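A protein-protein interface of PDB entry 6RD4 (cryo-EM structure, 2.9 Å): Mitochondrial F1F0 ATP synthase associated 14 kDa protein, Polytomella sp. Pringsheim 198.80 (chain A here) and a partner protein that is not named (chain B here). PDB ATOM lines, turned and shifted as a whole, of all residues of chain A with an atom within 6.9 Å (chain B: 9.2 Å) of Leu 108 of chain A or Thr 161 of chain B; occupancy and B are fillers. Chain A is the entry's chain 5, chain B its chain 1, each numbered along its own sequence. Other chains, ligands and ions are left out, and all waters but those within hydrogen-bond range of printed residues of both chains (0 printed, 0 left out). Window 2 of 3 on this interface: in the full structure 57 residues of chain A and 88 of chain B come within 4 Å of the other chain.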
ATOM      1  N   TYR A 103      19.158 -11.206  -3.061  1.00  0.00           N
ATOM      2  CA  TYR A 103      19.256 -11.196  -4.510  1.00  0.00           C
ATOM      3  C   TYR A 103      20.653 -10.834  -4.942  1.00  0.00           C
ATOM      4  O   TYR A 103      21.185 -11.449  -5.862  1.00  0.00           O
ATOM      5  CB  TYR A 103      18.276 -10.216  -5.145  1.00  0.00           C
ATOM      6  CG  TYR A 103      18.410 -10.133  -6.652  1.00  0.00           C
ATOM      7  CD1 TYR A 103      17.853 -11.083  -7.457  1.00  0.00           C
ATOM      8  CD2 TYR A 103      19.109  -9.106  -7.261  1.00  0.00           C
ATOM      9  CE1 TYR A 103      17.968 -11.016  -8.797  1.00  0.00           C
ATOM     10  CE2 TYR A 103      19.250  -9.062  -8.605  1.00  0.00           C
ATOM     11  CZ  TYR A 103      18.673 -10.014  -9.363  1.00  0.00           C
ATOM     12  OH  TYR A 103      18.795  -9.973 -10.716  1.00  0.00           O
ATOM     13  N   ASP A 104      21.239  -9.814  -4.319  1.00  0.00           N
ATOM     14  CA  ASP A 104      22.529  -9.306  -4.757  1.00  0.00           C
ATOM     15  C   ASP A 104      23.601 -10.359  -4.620  1.00  0.00           C
ATOM     16  O   ASP A 104      24.294 -10.679  -5.580  1.00  0.00           O
ATOM     17  CB  ASP A 104      22.913  -8.079  -3.955  1.00  0.00           C
ATOM     18  CG  ASP A 104      22.198  -6.858  -4.407  1.00  0.00           C
ATOM     19  OD1 ASP A 104      21.393  -6.976  -5.342  1.00  0.00           O
ATOM     20  OD2 ASP A 104      22.425  -5.780  -3.828  1.00  0.00           O
ATOM     21  N   ALA A 105      23.689 -10.972  -3.460  1.00  0.00           N
ATOM     22  CA  ALA A 105      24.791 -11.869  -3.217  1.00  0.00           C
ATOM     23  C   ALA A 105      24.607 -13.213  -3.885  1.00  0.00           C
ATOM     24  O   ALA A 105      25.596 -13.870  -4.191  1.00  0.00           O
ATOM     25  CB  ALA A 105      24.967 -12.051  -1.733  1.00  0.00           C
ATOM     26  N   LEU A 106      23.384 -13.650  -4.142  1.00  0.00           N
ATOM     27  CA  LEU A 106      23.195 -15.074  -4.355  1.00  0.00           C
ATOM     28  C   LEU A 106      22.361 -15.393  -5.577  1.00  0.00           C
ATOM     29  O   LEU A 106      21.653 -16.398  -5.589  1.00  0.00           O
ATOM     30  CB  LEU A 106      22.509 -15.711  -3.162  1.00  0.00           C
ATOM     31  CG  LEU A 106      23.041 -15.553  -1.765  1.00  0.00           C
ATOM     32  CD1 LEU A 106      21.956 -15.980  -0.870  1.00  0.00           C
ATOM     33  CD2 LEU A 106      24.211 -16.425  -1.570  1.00  0.00           C
ATOM     34  N   ASN A 107      22.444 -14.617  -6.650  1.00  0.00           N
ATOM     35  CA  ASN A 107      21.477 -14.872  -7.712  1.00  0.00           C
ATOM     36  C   ASN A 107      22.007 -15.567  -8.948  1.00  0.00           C
ATOM     37  O   ASN A 107      21.314 -16.450  -9.458  1.00  0.00           O
ATOM     38  CB  ASN A 107      20.816 -13.600  -8.188  1.00  0.00           C
ATOM     39  CG  ASN A 107      19.595 -13.885  -8.991  1.00  0.00           C
ATOM     40  OD1 ASN A 107      18.572 -14.252  -8.455  1.00  0.00           O
ATOM     41  ND2 ASN A 107      19.682 -13.688 -10.285  1.00  0.00           N
ATOM     42  N   LEU A 108      23.198 -15.182  -9.420  1.00  0.00           N
ATOM     43  CA  LEU A 108      23.938 -15.473 -10.668  1.00  0.00           C
ATOM     44  C   LEU A 108      23.628 -14.496 -11.783  1.00  0.00           C
ATOM     45  O   LEU A 108      24.273 -14.569 -12.809  1.00  0.00           O
ATOM     46  CB  LEU A 108      23.748 -16.879 -11.257  1.00  0.00           C
ATOM     47  CG  LEU A 108      24.211 -17.983 -10.328  1.00  0.00           C
ATOM     48  CD1 LEU A 108      23.878 -19.352 -10.890  1.00  0.00           C
ATOM     49  CD2 LEU A 108      25.690 -17.829 -10.093  1.00  0.00           C
ATOM     50  N   GLN A 109      22.690 -13.583 -11.618  1.00  0.00           N
ATOM     51  CA  GLN A 109      22.535 -12.508 -12.575  1.00  0.00           C
ATOM     52  C   GLN A 109      22.766 -11.152 -11.955  1.00  0.00           C
ATOM     53  O   GLN A 109      22.631 -10.144 -12.647  1.00  0.00           O
ATOM     54  CB  GLN A 109      21.149 -12.515 -13.222  1.00  0.00           C
ATOM     55  CG  GLN A 109      21.026 -13.331 -14.481  1.00  0.00           C
ATOM     56  CD  GLN A 109      20.847 -14.788 -14.207  1.00  0.00           C
ATOM     57  OE1 GLN A 109      21.649 -15.612 -14.633  1.00  0.00           O
ATOM     58  NE2 GLN A 109      19.788 -15.124 -13.494  1.00  0.00           N
ATOM     59  N   SER A 110      23.101 -11.095 -10.681  1.00  0.00           N
ATOM     60  CA  SER A 110      23.320  -9.830 -10.022  1.00  0.00           C
ATOM     61  C   SER A 110      24.657  -9.243 -10.424  1.00  0.00           C
ATOM     62  O   SER A 110      25.558  -9.941 -10.840  1.00  0.00           O
ATOM     63  CB  SER A 110      23.275 -10.022  -8.526  1.00  0.00           C
ATOM     64  OG  SER A 110      23.661  -8.841  -7.869  1.00  0.00           O
ATOM     65  N   LYS A 111      24.794  -7.943 -10.272  1.00  0.00           N
ATOM     66  CA  LYS A 111      26.083  -7.355 -10.583  1.00  0.00           C
ATOM     67  C   LYS A 111      27.095  -7.578  -9.480  1.00  0.00           C
ATOM     68  O   LYS A 111      28.283  -7.357  -9.705  1.00  0.00           O
ATOM     69  CB  LYS A 111      25.942  -5.865 -10.856  1.00  0.00           C
ATOM     70  CG  LYS A 111      25.026  -5.536 -12.006  1.00  0.00           C
ATOM     71  CD  LYS A 111      25.420  -6.278 -13.260  1.00  0.00           C
ATOM     72  CE  LYS A 111      24.385  -6.115 -14.355  1.00  0.00           C
ATOM     73  NZ  LYS A 111      24.661  -7.000 -15.514  1.00  0.00           N
ATOM     74  N   VAL A 113      27.665 -10.701  -7.329  1.00  0.00           N
ATOM     75  CA  VAL A 113      27.370 -12.042  -6.854  1.00  0.00           C
ATOM     76  C   VAL A 113      28.540 -12.462  -5.997  1.00  0.00           C
ATOM     77  O   VAL A 113      29.667 -12.019  -6.219  1.00  0.00           O
ATOM     78  CB  VAL A 113      27.180 -13.041  -8.004  1.00  0.00           C
ATOM     79  CG1 VAL A 113      26.335 -14.189  -7.568  1.00  0.00           C
ATOM     80  CG2 VAL A 113      26.617 -12.423  -9.143  1.00  0.00           C
ATOM     81  N   ILE A 115      29.517 -15.554  -6.054  1.00  0.00           N
ATOM     82  CA  ILE A 115      29.918 -16.873  -6.521  1.00  0.00           C
ATOM     83  C   ILE A 115      31.351 -16.881  -7.019  1.00  0.00           C
ATOM     84  O   ILE A 115      32.001 -17.924  -7.007  1.00  0.00           O
ATOM     85  CB  ILE A 115      28.920 -17.377  -7.580  1.00  0.00           C
ATOM     86  CG1 ILE A 115      29.082 -18.864  -7.841  1.00  0.00           C
ATOM     87  CG2 ILE A 115      29.063 -16.632  -8.861  1.00  0.00           C
ATOM     88  CD1 ILE A 115      28.827 -19.693  -6.648  1.00  0.00           C
ATOM     89  N   TRP A 116      31.899 -15.742  -7.401  1.00  0.00           N
ATOM     90  CA  TRP A 116      33.287 -15.693  -7.807  1.00  0.00           C
ATOM     91  C   TRP A 116      34.181 -15.308  -6.661  1.00  0.00           C
ATOM     92  O   TRP A 116      35.399 -15.330  -6.803  1.00  0.00           O
ATOM     93  CB  TRP A 116      33.464 -14.717  -8.962  1.00  0.00           C
ATOM     94  CG  TRP A 116      32.426 -14.884  -9.979  1.00  0.00           C
ATOM     95  CD1 TRP A 116      31.416 -14.040 -10.241  1.00  0.00           C
ATOM     96  CD2 TRP A 116      32.270 -15.987 -10.863  1.00  0.00           C
ATOM     97  NE1 TRP A 116      30.635 -14.533 -11.236  1.00  0.00           N
ATOM     98  CE2 TRP A 116      31.139 -15.738 -11.632  1.00  0.00           C
ATOM     99  CE3 TRP A 116      32.981 -17.164 -11.076  1.00  0.00           C
ATOM    100  CZ2 TRP A 116      30.705 -16.608 -12.603  1.00  0.00           C
ATOM    101  CZ3 TRP A 116      32.544 -18.027 -12.030  1.00  0.00           C
ATOM    102  CH2 TRP A 116      31.420 -17.750 -12.784  1.00  0.00           C
ATOM    103  N   PRO B 154      13.019 -16.262   1.011  1.00  0.00           N
ATOM    104  CA  PRO B 154      13.395 -16.957  -0.213  1.00  0.00           C
ATOM    105  C   PRO B 154      14.205 -18.198   0.088  1.00  0.00           C
ATOM    106  O   PRO B 154      15.058 -18.201   0.971  1.00  0.00           O
ATOM    107  CB  PRO B 154      14.221 -15.924  -0.966  1.00  0.00           C
ATOM    108  CG  PRO B 154      14.617 -14.995   0.006  1.00  0.00           C
ATOM    109  CD  PRO B 154      13.573 -14.908   1.017  1.00  0.00           C
ATOM    110  N   GLU B 155      13.909 -19.261  -0.646  1.00  0.00           N
ATOM    111  CA  GLU B 155      14.533 -20.548  -0.399  1.00  0.00           C
ATOM    112  C   GLU B 155      15.978 -20.519  -0.851  1.00  0.00           C
ATOM    113  O   GLU B 155      16.271 -20.207  -2.007  1.00  0.00           O
ATOM    114  CB  GLU B 155      13.776 -21.641  -1.133  1.00  0.00           C
ATOM    115  CG  GLU B 155      14.248 -23.016  -0.811  1.00  0.00           C
ATOM    116  CD  GLU B 155      14.081 -23.955  -1.973  1.00  0.00           C
ATOM    117  OE1 GLU B 155      14.263 -23.511  -3.122  1.00  0.00           O
ATOM    118  OE2 GLU B 155      13.750 -25.134  -1.747  1.00  0.00           O
ATOM    119  N   TRP B 156      16.880 -20.835   0.066  1.00  0.00           N
ATOM    120  CA  TRP B 156      18.309 -20.822  -0.174  1.00  0.00           C
ATOM    121  C   TRP B 156      18.857 -22.137   0.332  1.00  0.00           C
ATOM    122  O   TRP B 156      18.754 -22.430   1.523  1.00  0.00           O
ATOM    123  CB  TRP B 156      18.964 -19.648   0.538  1.00  0.00           C
ATOM    124  CG  TRP B 156      20.417 -19.556   0.362  1.00  0.00           C
ATOM    125  CD1 TRP B 156      21.134 -19.991  -0.688  1.00  0.00           C
ATOM    126  CD2 TRP B 156      21.350 -18.975   1.268  1.00  0.00           C
ATOM    127  NE1 TRP B 156      22.453 -19.738  -0.499  1.00  0.00           N
ATOM    128  CE2 TRP B 156      22.610 -19.108   0.701  1.00  0.00           C
ATOM    129  CE3 TRP B 156      21.236 -18.355   2.504  1.00  0.00           C
ATOM    130  CZ2 TRP B 156      23.744 -18.649   1.320  1.00  0.00           C
ATOM    131  CZ3 TRP B 156      22.359 -17.904   3.112  1.00  0.00           C
ATOM    132  CH2 TRP B 156      23.596 -18.045   2.524  1.00  0.00           C
ATOM    133  N   LYS B 157      19.417 -22.933  -0.567  1.00  0.00           N
ATOM    134  CA  LYS B 157      20.022 -24.201  -0.209  1.00  0.00           C
ATOM    135  C   LYS B 157      21.480 -23.960   0.162  1.00  0.00           C
ATOM    136  O   LYS B 157      21.941 -22.823   0.171  1.00  0.00           O
ATOM    137  CB  LYS B 157      19.859 -25.179  -1.350  1.00  0.00           C
ATOM    138  CG  LYS B 157      18.436 -25.455  -1.704  1.00  0.00           C
ATOM    139  CD  LYS B 157      17.737 -26.031  -0.519  1.00  0.00           C
ATOM    140  CE  LYS B 157      16.511 -26.781  -0.923  1.00  0.00           C
ATOM    141  NZ  LYS B 157      16.080 -27.635   0.207  1.00  0.00           N
ATOM    142  N   LYS B 158      22.234 -25.023   0.440  1.00  0.00           N
ATOM    143  CA  LYS B 158      23.511 -24.867   1.135  1.00  0.00           C
ATOM    144  C   LYS B 158      24.584 -24.282   0.231  1.00  0.00           C
ATOM    145  O   LYS B 158      25.209 -23.271   0.561  1.00  0.00           O
ATOM    146  CB  LYS B 158      23.963 -26.204   1.704  1.00  0.00           C
ATOM    147  CG  LYS B 158      25.211 -26.123   2.546  1.00  0.00           C
ATOM    148  CD  LYS B 158      24.993 -25.295   3.764  1.00  0.00           C
ATOM    149  CE  LYS B 158      25.784 -25.810   4.931  1.00  0.00           C
ATOM    150  NZ  LYS B 158      25.418 -27.184   5.309  1.00  0.00           N
ATOM    151  N   GLY B 159      24.826 -24.905  -0.913  1.00  0.00           N
ATOM    152  CA  GLY B 159      25.785 -24.376  -1.850  1.00  0.00           C
ATOM    153  C   GLY B 159      25.156 -23.803  -3.090  1.00  0.00           C
ATOM    154  O   GLY B 159      25.880 -23.464  -4.035  1.00  0.00           O
ATOM    155  N   LYS B 160      23.848 -23.682  -3.132  1.00  0.00           N
ATOM    156  CA  LYS B 160      23.162 -23.320  -4.351  1.00  0.00           C
ATOM    157  C   LYS B 160      22.998 -21.814  -4.414  1.00  0.00           C
ATOM    158  O   LYS B 160      23.590 -21.063  -3.639  1.00  0.00           O
ATOM    159  CB  LYS B 160      21.836 -24.050  -4.420  1.00  0.00           C
ATOM    160  CG  LYS B 160      21.975 -25.530  -4.263  1.00  0.00           C
ATOM    161  CD  LYS B 160      22.870 -26.092  -5.315  1.00  0.00           C
ATOM    162  CE  LYS B 160      23.185 -27.529  -5.035  1.00  0.00           C
ATOM    163  NZ  LYS B 160      24.193 -28.011  -5.995  1.00  0.00           N
ATOM    164  N   THR B 161      22.201 -21.359  -5.357  1.00  0.00           N
ATOM    165  CA  THR B 161      21.883 -19.959  -5.486  1.00  0.00           C
ATOM    166  C   THR B 161      20.391 -19.774  -5.300  1.00  0.00           C
ATOM    167  O   THR B 161      19.649 -20.719  -5.036  1.00  0.00           O
ATOM    168  CB  THR B 161      22.327 -19.421  -6.836  1.00  0.00           C
ATOM    169  OG1 THR B 161      21.919 -20.336  -7.852  1.00  0.00           O
ATOM    170  CG2 THR B 161      23.821 -19.279  -6.854  1.00  0.00           C
ATOM    171  N   VAL B 162      19.963 -18.529  -5.412  1.00  0.00           N
ATOM    172  CA  VAL B 162      18.580 -18.152  -5.195  1.00  0.00           C
ATOM    173  C   VAL B 162      18.032 -17.662  -6.521  1.00  0.00           C
ATOM    174  O   VAL B 162      18.585 -16.739  -7.119  1.00  0.00           O
ATOM    175  CB  VAL B 162      18.463 -17.084  -4.102  1.00  0.00           C
ATOM    176  CG1 VAL B 162      17.078 -16.667  -3.972  1.00  0.00           C
ATOM    177  CG2 VAL B 162      18.901 -17.643  -2.798  1.00  0.00           C
ATOM    178  N   SER B 163      16.972 -18.295  -6.999  1.00  0.00           N
ATOM    179  CA  SER B 163      16.367 -17.899  -8.257  1.00  0.00           C
ATOM    180  C   SER B 163      15.503 -16.678  -8.051  1.00  0.00           C
ATOM    181  O   SER B 163      14.963 -16.455  -6.975  1.00  0.00           O
ATOM    182  CB  SER B 163      15.528 -19.031  -8.828  1.00  0.00           C
ATOM    183  OG  SER B 163      14.610 -19.499  -7.867  1.00  0.00           O
ATOM    184  N   ILE B 164      15.360 -15.879  -9.105  1.00  0.00           N
ATOM    185  CA  ILE B 164      14.477 -14.729  -8.992  1.00  0.00           C
ATOM    186  C   ILE B 164      13.027 -15.155  -9.109  1.00  0.00           C
ATOM    187  O   ILE B 164      12.140 -14.436  -8.658  1.00  0.00           O
ATOM    188  CB  ILE B 164      14.829 -13.643 -10.016  1.00  0.00           C
ATOM    189  CG1 ILE B 164      14.338 -12.287  -9.538  1.00  0.00           C
ATOM    190  CG2 ILE B 164      14.223 -13.936 -11.347  1.00  0.00           C
ATOM    191  CD1 ILE B 164      14.767 -11.174 -10.389  1.00  0.00           C
ATOM    192  N   ASN B 166      11.873 -17.383  -7.275  1.00  0.00           N
ATOM    193  CA  ASN B 166      11.497 -17.659  -5.901  1.00  0.00           C
ATOM    194  C   ASN B 166      11.569 -16.422  -5.031  1.00  0.00           C
ATOM    195  O   ASN B 166      10.856 -16.330  -4.034  1.00  0.00           O
ATOM    196  CB  ASN B 166      12.388 -18.742  -5.315  1.00  0.00           C
ATOM    197  CG  ASN B 166      11.906 -19.214  -3.987  1.00  0.00           C
ATOM    198  OD1 ASN B 166      12.449 -18.849  -2.958  1.00  0.00           O
ATOM    199  ND2 ASN B 166      10.856 -20.012  -3.995  1.00  0.00           N
ATOM    200  N   LEU B 167      12.425 -15.469  -5.379  1.00  0.00           N
ATOM    201  CA  LEU B 167      12.403 -14.180  -4.713  1.00  0.00           C
ATOM    202  C   LEU B 167      11.147 -13.410  -5.045  1.00  0.00           C
ATOM    203  O   LEU B 167      10.732 -12.549  -4.275  1.00  0.00           O
ATOM    204  CB  LEU B 167      13.618 -13.365  -5.116  1.00  0.00           C
ATOM    205  CG  LEU B 167      14.946 -13.733  -4.499  1.00  0.00           C
ATOM    206  CD1 LEU B 167      16.012 -13.171  -5.319  1.00  0.00           C
ATOM    207  CD2 LEU B 167      15.030 -13.098  -3.170  1.00  0.00           C
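The backbone NH of Val 162 of chain B sits at hydrogen-bond distance from the backbone carbonyl oxygen of Leu 106 of chain A, at 2.7 Å. The side-chain amide oxygen (OD1) of Asn 107 of chain A sits close to the backbone carbonyl oxygen (O) of Val 162 of chain B, at 2.8 Å.
ND2 of Asn 107 of chain A lies close to N of Gln 109 of chain A (3.3 Å).
Ile 164 of chain B touches Tyr 103 of chain A (CD1 to CE1, 3.6 Å). Leu 167 of chain B touches Tyr 103 of chain A. Leu 106 of chain A touches Trp 156 of chain B (CD1 to CE2, 3.6 Å). Leu 106 of chain A touches Thr 161 of chain B (O to CB, 3.3 Å). C of Ser 163 of chain B touches OD1 of Asn 107 of chain A (3.9 Å). OD1 of Asn 107 of chain A touches N of Ile 164 of chain B, at 3.7 Å. Thr 161 of chain B touches Leu 108 of chain A.
Leu 108 of chain A touches just one residue of chain B: Thr 161. No residue of chain B comes within 4 Å of Gln 109 of chain A. Printed residues of chain A within 4 Å of Ser 163 of chain B: Asn 107. Of the printed residues of chain B, Tyr 103 of chain A touches Ile 164 and Leu 167. Printed residues of chain A within 4 Å of Val 162 of chain B: Leu 106 (2.7 Å) and Asn 107 (2.8 Å). Of the printed residues of chain A, Ile 164 of chain B touches Tyr 103 (3.6 Å) and Asn 107 (3.7 Å). Printed residues of chain B within 4 Å of Leu 106 of chain A: Trp 156 (3.6 Å), Thr 161 (3.3 Å) and Val 162 (2.7 Å). The nearest residue of chain A that does not touch Thr 161 of chain B is Asn 107 of chain A (4.1 Å). The nearest printed residue of chain B that does not touch Leu 106 of chain A is Lys 160 of chain B (5.1 Å).
Of the 12 printed residues of chain A, 4 touch a printed residue of chain B. Hydrophobic or aromatic side chains of chain A within 4 Å of the printed part of chain B: Tyr 103, Leu 106 and Leu 108. Of the 13 printed residues of chain B, 6 touch a printed residue of chain A. Among the printed residues, no Asp or Glu carboxylate lies within 4 Å of a Lys or Arg side-chain nitrogen of the other chain.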
